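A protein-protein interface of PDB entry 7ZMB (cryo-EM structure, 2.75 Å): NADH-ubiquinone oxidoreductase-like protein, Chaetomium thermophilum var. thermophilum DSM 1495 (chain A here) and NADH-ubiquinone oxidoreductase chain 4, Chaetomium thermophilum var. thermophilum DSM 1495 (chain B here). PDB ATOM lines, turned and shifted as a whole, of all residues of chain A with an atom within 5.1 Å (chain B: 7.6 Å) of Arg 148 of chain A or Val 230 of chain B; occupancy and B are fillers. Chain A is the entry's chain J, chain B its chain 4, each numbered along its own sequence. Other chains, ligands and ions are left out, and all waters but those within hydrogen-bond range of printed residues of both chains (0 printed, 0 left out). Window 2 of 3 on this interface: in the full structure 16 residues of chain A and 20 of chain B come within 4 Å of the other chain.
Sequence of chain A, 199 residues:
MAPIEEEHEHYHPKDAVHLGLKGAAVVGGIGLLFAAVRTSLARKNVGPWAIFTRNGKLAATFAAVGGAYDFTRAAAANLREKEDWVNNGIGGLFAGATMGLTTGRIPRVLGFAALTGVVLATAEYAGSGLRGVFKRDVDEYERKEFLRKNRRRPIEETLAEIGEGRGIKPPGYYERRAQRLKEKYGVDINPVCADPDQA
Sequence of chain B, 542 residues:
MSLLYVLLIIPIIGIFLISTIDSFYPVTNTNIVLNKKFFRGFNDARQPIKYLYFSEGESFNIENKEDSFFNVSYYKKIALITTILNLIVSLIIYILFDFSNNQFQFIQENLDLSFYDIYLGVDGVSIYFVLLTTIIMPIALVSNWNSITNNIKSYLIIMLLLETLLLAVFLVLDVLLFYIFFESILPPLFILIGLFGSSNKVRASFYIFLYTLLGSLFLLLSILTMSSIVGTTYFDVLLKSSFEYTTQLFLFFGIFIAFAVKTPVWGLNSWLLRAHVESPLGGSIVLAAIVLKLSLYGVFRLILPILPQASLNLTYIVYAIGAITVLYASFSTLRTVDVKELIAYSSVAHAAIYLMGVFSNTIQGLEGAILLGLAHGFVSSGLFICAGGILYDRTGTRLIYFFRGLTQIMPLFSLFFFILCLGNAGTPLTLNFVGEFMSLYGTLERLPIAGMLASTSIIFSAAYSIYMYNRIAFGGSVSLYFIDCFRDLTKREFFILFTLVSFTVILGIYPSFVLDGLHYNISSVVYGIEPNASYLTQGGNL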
ATOM      1  N   LYS A 144     -11.722 -12.283   0.792  1.00  0.00           N
ATOM      2  CA  LYS A 144     -10.515 -12.866   0.224  1.00  0.00           C
ATOM      3  C   LYS A 144      -9.270 -12.284   0.868  1.00  0.00           C
ATOM      4  O   LYS A 144      -8.294 -13.000   1.107  1.00  0.00           O
ATOM      5  CB  LYS A 144     -10.499 -12.647  -1.285  1.00  0.00           C
ATOM      6  CG  LYS A 144     -11.646 -13.318  -2.003  1.00  0.00           C
ATOM      7  CD  LYS A 144     -11.624 -14.810  -1.779  1.00  0.00           C
ATOM      8  CE  LYS A 144     -12.225 -15.552  -2.957  1.00  0.00           C
ATOM      9  NZ  LYS A 144     -11.363 -15.456  -4.161  1.00  0.00           N
ATOM     10  N   GLU A 145      -9.286 -10.981   1.150  1.00  0.00           N
ATOM     11  CA  GLU A 145      -8.140 -10.344   1.789  1.00  0.00           C
ATOM     12  C   GLU A 145      -7.933 -10.871   3.203  1.00  0.00           C
ATOM     13  O   GLU A 145      -6.792 -11.043   3.649  1.00  0.00           O
ATOM     14  CB  GLU A 145      -8.329  -8.828   1.787  1.00  0.00           C
ATOM     15  CG  GLU A 145      -7.126  -8.036   2.234  1.00  0.00           C
ATOM     16  CD  GLU A 145      -7.117  -7.789   3.732  1.00  0.00           C
ATOM     17  OE1 GLU A 145      -8.196  -7.877   4.358  1.00  0.00           O
ATOM     18  OE2 GLU A 145      -6.035  -7.506   4.282  1.00  0.00           O
ATOM     19  N   PHE A 146      -9.023 -11.144   3.924  1.00  0.00           N
ATOM     20  CA  PHE A 146      -8.884 -11.624   5.296  1.00  0.00           C
ATOM     21  C   PHE A 146      -8.374 -13.058   5.339  1.00  0.00           C
ATOM     22  O   PHE A 146      -7.470 -13.373   6.120  1.00  0.00           O
ATOM     23  CB  PHE A 146     -10.214 -11.501   6.038  1.00  0.00           C
ATOM     24  CG  PHE A 146     -10.217 -12.170   7.386  1.00  0.00           C
ATOM     25  CD1 PHE A 146      -9.188 -11.946   8.288  1.00  0.00           C
ATOM     26  CD2 PHE A 146     -11.249 -13.016   7.752  1.00  0.00           C
ATOM     27  CE1 PHE A 146      -9.183 -12.558   9.519  1.00  0.00           C
ATOM     28  CE2 PHE A 146     -11.252 -13.630   8.988  1.00  0.00           C
ATOM     29  CZ  PHE A 146     -10.217 -13.400   9.872  1.00  0.00           C
ATOM     30  N   LEU A 147      -8.927 -13.938   4.498  1.00  0.00           N
ATOM     31  CA  LEU A 147      -8.498 -15.334   4.469  1.00  0.00           C
ATOM     32  C   LEU A 147      -7.069 -15.518   3.994  1.00  0.00           C
ATOM     33  O   LEU A 147      -6.518 -16.611   4.159  1.00  0.00           O
ATOM     34  CB  LEU A 147      -9.412 -16.164   3.575  1.00  0.00           C
ATOM     35  CG  LEU A 147     -10.851 -16.364   3.993  1.00  0.00           C
ATOM     36  CD1 LEU A 147     -11.585 -17.084   2.904  1.00  0.00           C
ATOM     37  CD2 LEU A 147     -10.865 -17.177   5.255  1.00  0.00           C
ATOM     38  N   ARG A 148      -6.465 -14.493   3.413  1.00  0.00           N
ATOM     39  CA  ARG A 148      -5.140 -14.588   2.829  1.00  0.00           C
ATOM     40  C   ARG A 148      -4.049 -14.025   3.722  1.00  0.00           C
ATOM     41  O   ARG A 148      -2.903 -14.475   3.643  1.00  0.00           O
ATOM     42  CB  ARG A 148      -5.139 -13.851   1.492  1.00  0.00           C
ATOM     43  CG  ARG A 148      -3.870 -13.904   0.692  1.00  0.00           C
ATOM     44  CD  ARG A 148      -4.117 -13.097  -0.551  1.00  0.00           C
ATOM     45  NE  ARG A 148      -5.425 -13.444  -1.098  1.00  0.00           N
ATOM     46  CZ  ARG A 148      -5.926 -12.965  -2.228  1.00  0.00           C
ATOM     47  NH1 ARG A 148      -7.128 -13.349  -2.630  1.00  0.00           N
ATOM     48  NH2 ARG A 148      -5.224 -12.112  -2.958  1.00  0.00           N
ATOM     49  N   LYS A 149      -4.375 -13.057   4.573  1.00  0.00           N
ATOM     50  CA  LYS A 149      -3.383 -12.373   5.386  1.00  0.00           C
ATOM     51  C   LYS A 149      -3.549 -12.652   6.872  1.00  0.00           C
ATOM     52  O   LYS A 149      -2.871 -12.021   7.690  1.00  0.00           O
ATOM     53  CB  LYS A 149      -3.429 -10.869   5.116  1.00  0.00           C
ATOM     54  CG  LYS A 149      -3.020 -10.499   3.707  1.00  0.00           C
ATOM     55  CD  LYS A 149      -2.235  -9.197   3.668  1.00  0.00           C
ATOM     56  CE  LYS A 149      -2.923  -8.095   4.454  1.00  0.00           C
ATOM     57  NZ  LYS A 149      -2.359  -6.755   4.141  1.00  0.00           N
ATOM     58  N   ASN A 150      -4.426 -13.582   7.246  1.00  0.00           N
ATOM     59  CA  ASN A 150      -4.504 -14.056   8.628  1.00  0.00           C
ATOM     60  C   ASN A 150      -3.474 -15.173   8.819  1.00  0.00           C
ATOM     61  O   ASN A 150      -3.792 -16.323   9.125  1.00  0.00           O
ATOM     62  CB  ASN A 150      -5.914 -14.523   8.954  1.00  0.00           C
ATOM     63  CG  ASN A 150      -6.149 -14.666  10.442  1.00  0.00           C
ATOM     64  OD1 ASN A 150      -5.238 -14.476  11.246  1.00  0.00           O
ATOM     65  ND2 ASN A 150      -7.378 -14.999  10.818  1.00  0.00           N
ATOM     66  N   ARG A 151      -2.206 -14.804   8.631  1.00  0.00           N
ATOM     67  CA  ARG A 151      -1.121 -15.778   8.586  1.00  0.00           C
ATOM     68  C   ARG A 151      -0.719 -16.306   9.957  1.00  0.00           C
ATOM     69  O   ARG A 151      -0.265 -17.451  10.056  1.00  0.00           O
ATOM     70  CB  ARG A 151       0.100 -15.169   7.893  1.00  0.00           C
ATOM     71  CG  ARG A 151      -0.126 -14.908   6.420  1.00  0.00           C
ATOM     72  CD  ARG A 151       1.094 -14.308   5.757  1.00  0.00           C
ATOM     73  NE  ARG A 151       0.860 -14.085   4.339  1.00  0.00           N
ATOM     74  CZ  ARG A 151       0.375 -12.952   3.845  1.00  0.00           C
ATOM     75  NH1 ARG A 151       0.178 -12.819   2.542  1.00  0.00           N
ATOM     76  NH2 ARG A 151       0.089 -11.946   4.658  1.00  0.00           N
ATOM     77  N   LEU B 224      -7.132 -25.623  -7.206  1.00  0.00           N
ATOM     78  CA  LEU B 224      -7.897 -24.464  -7.637  1.00  0.00           C
ATOM     79  C   LEU B 224      -8.516 -23.739  -6.453  1.00  0.00           C
ATOM     80  O   LEU B 224      -8.591 -22.508  -6.446  1.00  0.00           O
ATOM     81  CB  LEU B 224      -8.962 -24.894  -8.644  1.00  0.00           C
ATOM     82  CG  LEU B 224      -8.369 -25.361  -9.969  1.00  0.00           C
ATOM     83  CD1 LEU B 224      -9.429 -25.553 -11.039  1.00  0.00           C
ATOM     84  CD2 LEU B 224      -7.296 -24.399 -10.422  1.00  0.00           C
ATOM     85  N   THR B 225      -8.961 -24.482  -5.443  1.00  0.00           N
ATOM     86  CA  THR B 225      -9.436 -23.858  -4.213  1.00  0.00           C
ATOM     87  C   THR B 225      -8.329 -23.066  -3.524  1.00  0.00           C
ATOM     88  O   THR B 225      -8.563 -21.951  -3.053  1.00  0.00           O
ATOM     89  CB  THR B 225     -10.009 -24.926  -3.284  1.00  0.00           C
ATOM     90  OG1 THR B 225     -11.199 -25.461  -3.865  1.00  0.00           O
ATOM     91  CG2 THR B 225     -10.333 -24.352  -1.921  1.00  0.00           C
ATOM     92  N   MET B 226      -7.114 -23.614  -3.466  1.00  0.00           N
ATOM     93  CA  MET B 226      -6.013 -22.882  -2.846  1.00  0.00           C
ATOM     94  C   MET B 226      -5.746 -21.572  -3.565  1.00  0.00           C
ATOM     95  O   MET B 226      -5.504 -20.545  -2.926  1.00  0.00           O
ATOM     96  CB  MET B 226      -4.733 -23.715  -2.847  1.00  0.00           C
ATOM     97  CG  MET B 226      -4.820 -25.040  -2.156  1.00  0.00           C
ATOM     98  SD  MET B 226      -3.174 -25.741  -2.091  1.00  0.00           S
ATOM     99  CE  MET B 226      -3.530 -27.362  -1.465  1.00  0.00           C
ATOM    100  N   SER B 227      -5.752 -21.598  -4.895  1.00  0.00           N
ATOM    101  CA  SER B 227      -5.408 -20.405  -5.645  1.00  0.00           C
ATOM    102  C   SER B 227      -6.463 -19.322  -5.484  1.00  0.00           C
ATOM    103  O   SER B 227      -6.137 -18.135  -5.525  1.00  0.00           O
ATOM    104  CB  SER B 227      -5.200 -20.752  -7.114  1.00  0.00           C
ATOM    105  OG  SER B 227      -4.471 -19.732  -7.768  1.00  0.00           O
ATOM    106  N   SER B 228      -7.722 -19.706  -5.295  1.00  0.00           N
ATOM    107  CA  SER B 228      -8.769 -18.723  -5.074  1.00  0.00           C
ATOM    108  C   SER B 228      -8.713 -18.119  -3.683  1.00  0.00           C
ATOM    109  O   SER B 228      -9.228 -17.016  -3.482  1.00  0.00           O
ATOM    110  CB  SER B 228     -10.139 -19.348  -5.311  1.00  0.00           C
ATOM    111  OG  SER B 228     -10.193 -20.634  -4.738  1.00  0.00           O
ATOM    112  N   ILE B 229      -8.105 -18.805  -2.722  1.00  0.00           N
ATOM    113  CA  ILE B 229      -7.936 -18.247  -1.386  1.00  0.00           C
ATOM    114  C   ILE B 229      -6.683 -17.390  -1.307  1.00  0.00           C
ATOM    115  O   ILE B 229      -6.725 -16.245  -0.857  1.00  0.00           O
ATOM    116  CB  ILE B 229      -7.921 -19.378  -0.335  1.00  0.00           C
ATOM    117  CG1 ILE B 229      -9.181 -20.237  -0.458  1.00  0.00           C
ATOM    118  CG2 ILE B 229      -7.849 -18.804   1.059  1.00  0.00           C
ATOM    119  CD1 ILE B 229      -9.207 -21.461   0.434  1.00  0.00           C
ATOM    120  N   VAL B 230      -5.558 -17.923  -1.776  1.00  0.00           N
ATOM    121  CA  VAL B 230      -4.282 -17.228  -1.683  1.00  0.00           C
ATOM    122  C   VAL B 230      -4.118 -16.203  -2.798  1.00  0.00           C
ATOM    123  O   VAL B 230      -3.408 -15.209  -2.634  1.00  0.00           O
ATOM    124  CB  VAL B 230      -3.147 -18.267  -1.685  1.00  0.00           C
ATOM    125  CG1 VAL B 230      -1.785 -17.616  -1.830  1.00  0.00           C
ATOM    126  CG2 VAL B 230      -3.202 -19.084  -0.428  1.00  0.00           C
ATOM    127  N   GLY B 231      -4.766 -16.405  -3.934  1.00  0.00           N
ATOM    128  CA  GLY B 231      -4.571 -15.531  -5.064  1.00  0.00           C
ATOM    129  C   GLY B 231      -3.399 -15.891  -5.940  1.00  0.00           C
ATOM    130  O   GLY B 231      -3.152 -15.196  -6.930  1.00  0.00           O
ATOM    131  N   THR B 232      -2.666 -16.941  -5.600  1.00  0.00           N
ATOM    132  CA  THR B 232      -1.569 -17.437  -6.410  1.00  0.00           C
ATOM    133  C   THR B 232      -1.283 -18.870  -5.997  1.00  0.00           C
ATOM    134  O   THR B 232      -1.950 -19.438  -5.129  1.00  0.00           O
ATOM    135  CB  THR B 232      -0.319 -16.559  -6.278  1.00  0.00           C
ATOM    136  OG1 THR B 232       0.758 -17.147  -7.014  1.00  0.00           O
ATOM    137  CG2 THR B 232       0.074 -16.406  -4.850  1.00  0.00           C
ATOM    138  N   THR B 233      -0.286 -19.454  -6.650  1.00  0.00           N
ATOM    139  CA  THR B 233       0.201 -20.782  -6.341  1.00  0.00           C
ATOM    140  C   THR B 233       1.702 -20.829  -6.117  1.00  0.00           C
ATOM    141  O   THR B 233       2.209 -21.878  -5.712  1.00  0.00           O
ATOM    142  CB  THR B 233      -0.168 -21.763  -7.467  1.00  0.00           C
ATOM    143  OG1 THR B 233       0.217 -21.208  -8.734  1.00  0.00           O
ATOM    144  CG2 THR B 233      -1.658 -22.090  -7.458  1.00  0.00           C
ATOM    145  N   TYR B 234       2.420 -19.734  -6.370  1.00  0.00           N
ATOM    146  CA  TYR B 234       3.866 -19.679  -6.200  1.00  0.00           C
ATOM    147  C   TYR B 234       4.257 -20.180  -4.820  1.00  0.00           C
ATOM    148  O   TYR B 234       3.665 -19.775  -3.818  1.00  0.00           O
ATOM    149  CB  TYR B 234       4.348 -18.241  -6.410  1.00  0.00           C
ATOM    150  CG  TYR B 234       5.849 -18.092  -6.520  1.00  0.00           C
ATOM    151  CD1 TYR B 234       6.542 -18.605  -7.610  1.00  0.00           C
ATOM    152  CD2 TYR B 234       6.569 -17.430  -5.542  1.00  0.00           C
ATOM    153  CE1 TYR B 234       7.900 -18.466  -7.713  1.00  0.00           C
ATOM    154  CE2 TYR B 234       7.928 -17.289  -5.636  1.00  0.00           C
ATOM    155  CZ  TYR B 234       8.592 -17.811  -6.720  1.00  0.00           C
ATOM    156  OH  TYR B 234       9.955 -17.665  -6.807  1.00  0.00           O
ATOM    157  N   VAL B 237       4.949 -17.640  -1.900  1.00  0.00           N
ATOM    158  CA  VAL B 237       3.740 -16.976  -1.425  1.00  0.00           C
ATOM    159  C   VAL B 237       2.799 -17.972  -0.760  1.00  0.00           C
ATOM    160  O   VAL B 237       2.239 -17.700   0.304  1.00  0.00           O
ATOM    161  CB  VAL B 237       3.043 -16.249  -2.586  1.00  0.00           C
ATOM    162  CG1 VAL B 237       1.856 -15.461  -2.074  1.00  0.00           C
ATOM    163  CG2 VAL B 237       4.026 -15.370  -3.327  1.00  0.00           C
ATOM    164  N   LEU B 238       2.609 -19.137  -1.373  1.00  0.00           N
ATOM    165  CA  LEU B 238       1.550 -20.039  -0.931  1.00  0.00           C
ATOM    166  C   LEU B 238       1.891 -20.735   0.377  1.00  0.00           C
ATOM    167  O   LEU B 238       0.996 -20.998   1.183  1.00  0.00           O
ATOM    168  CB  LEU B 238       1.255 -21.059  -2.028  1.00  0.00           C
ATOM    169  CG  LEU B 238       0.285 -22.208  -1.758  1.00  0.00           C
ATOM    170  CD1 LEU B 238      -1.144 -21.740  -1.834  1.00  0.00           C
ATOM    171  CD2 LEU B 238       0.535 -23.318  -2.744  1.00  0.00           C
ATOM    172  N   LEU B 239       3.168 -21.031   0.612  1.00  0.00           N
ATOM    173  CA  LEU B 239       3.550 -21.793   1.796  1.00  0.00           C
ATOM    174  C   LEU B 239       3.224 -21.041   3.082  1.00  0.00           C
ATOM    175  O   LEU B 239       2.751 -21.638   4.056  1.00  0.00           O
ATOM    176  CB  LEU B 239       5.038 -22.125   1.741  1.00  0.00           C
ATOM    177  CG  LEU B 239       5.458 -23.189   0.731  1.00  0.00           C
ATOM    178  CD1 LEU B 239       6.877 -23.640   0.982  1.00  0.00           C
ATOM    179  CD2 LEU B 239       4.493 -24.348   0.745  1.00  0.00           C
ATOM    180  N   LYS B 240       3.473 -19.735   3.106  1.00  0.00           N
ATOM    181  CA  LYS B 240       3.229 -18.892   4.269  1.00  0.00           C
ATOM    182  C   LYS B 240       1.758 -18.567   4.498  1.00  0.00           C
ATOM    183  O   LYS B 240       1.432 -17.925   5.500  1.00  0.00           O
ATOM    184  CB  LYS B 240       4.056 -17.612   4.137  1.00  0.00           C
ATOM    185  CG  LYS B 240       3.619 -16.720   3.008  1.00  0.00           C
ATOM    186  CD  LYS B 240       4.491 -15.490   2.911  1.00  0.00           C
ATOM    187  CE  LYS B 240       4.068 -14.637   1.739  1.00  0.00           C
ATOM    188  NZ  LYS B 240       2.719 -14.051   1.925  1.00  0.00           N
ATOM    189  N   SER B 241       0.863 -18.986   3.617  1.00  0.00           N
ATOM    190  CA  SER B 241      -0.559 -18.872   3.900  1.00  0.00           C
ATOM    191  C   SER B 241      -1.008 -20.014   4.796  1.00  0.00           C
ATOM    192  O   SER B 241      -0.609 -21.161   4.605  1.00  0.00           O
ATOM    193  CB  SER B 241      -1.371 -18.878   2.608  1.00  0.00           C
ATOM    194  OG  SER B 241      -1.339 -17.613   1.972  1.00  0.00           O
ATOM    195  N   SER B 242      -1.833 -19.691   5.779  1.00  0.00           N
ATOM    196  CA  SER B 242      -2.513 -20.696   6.577  1.00  0.00           C
ATOM    197  C   SER B 242      -3.911 -20.944   6.020  1.00  0.00           C
ATOM    198  O   SER B 242      -4.381 -20.259   5.110  1.00  0.00           O
ATOM    199  CB  SER B 242      -2.582 -20.271   8.044  1.00  0.00           C
ATOM    200  OG  SER B 242      -1.294 -20.248   8.627  1.00  0.00           O
ATOM    201  N   PHE B 243      -4.573 -21.953   6.571  1.00  0.00           N
ATOM    202  CA  PHE B 243      -5.880 -22.349   6.087  1.00  0.00           C
ATOM    203  C   PHE B 243      -6.756 -22.737   7.263  1.00  0.00           C
ATOM    204  O   PHE B 243      -6.268 -23.212   8.290  1.00  0.00           O
ATOM    205  CB  PHE B 243      -5.781 -23.505   5.090  1.00  0.00           C
ATOM    206  CG  PHE B 243      -5.372 -23.078   3.719  1.00  0.00           C
ATOM    207  CD1 PHE B 243      -6.145 -22.173   3.009  1.00  0.00           C
ATOM    208  CD2 PHE B 243      -4.216 -23.558   3.145  1.00  0.00           C
ATOM    209  CE1 PHE B 243      -5.772 -21.767   1.754  1.00  0.00           C
ATOM    210  CE2 PHE B 243      -3.842 -23.151   1.887  1.00  0.00           C
ATOM    211  CZ  PHE B 243      -4.625 -22.257   1.191  1.00  0.00           C
ATOM    212  N   ILE B 306       1.418 -26.875   3.704  1.00  0.00           N
ATOM    213  CA  ILE B 306       0.215 -26.056   3.618  1.00  0.00           C
ATOM    214  C   ILE B 306      -1.009 -26.703   4.253  1.00  0.00           C
ATOM    215  O   ILE B 306      -2.032 -26.019   4.407  1.00  0.00           O
ATOM    216  CB  ILE B 306      -0.087 -25.646   2.160  1.00  0.00           C
ATOM    217  CG1 ILE B 306      -0.076 -26.855   1.232  1.00  0.00           C
ATOM    218  CG2 ILE B 306       0.952 -24.681   1.673  1.00  0.00           C
ATOM    219  CD1 ILE B 306      -0.256 -26.499  -0.220  1.00  0.00           C
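The side-chain amino group (NZ) of Lys 144 of chain A lies within hydrogen-bond range of the backbone carbonyl oxygen (O) of Ser 228 of chain B, 2.7 Å away.
O of Ile 229 of chain B is in hydrogen-bond range of NE of Arg 148 of chain A, 3.1 Å away.
The backbone carbonyl oxygen (O) of Val 230 of chain B sits close to the guanidinium group (NE) of Arg 148 of chain A, at 3.1 Å.
The backbone carbonyl oxygen (O) of Arg 151 of chain A is in hydrogen-bond range of the side-chain hydroxyl (OG) of Ser 242 of chain B (3.3 Å).
The guanidinium group (NH1) of Arg 151 of chain A lies close to the side-chain amino group (NZ) of Lys 240 of chain B.
OG of Ser 228 of chain B is in hydrogen-bond range of O of Leu 224 of chain B (3.0 Å).
The side-chain hydroxyl of Ser 228 of chain B lies within hydrogen-bond range of the backbone carbonyl oxygen of Thr 225 of chain B, 2.7 Å away.
Among the printed residues, merely in contact across the chains: Leu 147 of chain A with Ile 229 of chain B (3.97 Å) and Arg 148 of chain A with Ser 241 of chain B (3.9 Å).
Of the printed residues of chain B, Lys 144 of chain A touches Ser 228 (2.7 Å).
Printed residues of chain B within 4 Å of Leu 147 of chain A: Ile 229.
Of the printed residues of chain B, Arg 148 of chain A touches Ile 229, Val 230 and Ser 241.
Printed residues of chain A within 4 Å of Ser 228 of chain B: Lys 144 (2.7 Å).
Val 230 of chain B touches just one residue of chain A: Arg 148.
Val 237 of chain B touches none of the printed residues of chain A.
Printed residues of chain A within 4 Å of Ser 242 of chain B: Arg 151.
The nearest printed residue of chain B that does not touch Arg 148 of chain A is Gly 231 of chain B (4.01 Å).
The nearest printed residue of chain A that does not touch Val 230 of chain B is Leu 147 of chain A (6.2 Å).
Along chain A the printed residues that touch a printed residue of chain B span positions 144 to 151.
Hydrophobic or aromatic side chains of chain B that line the printed part of chain A: Ile 229.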
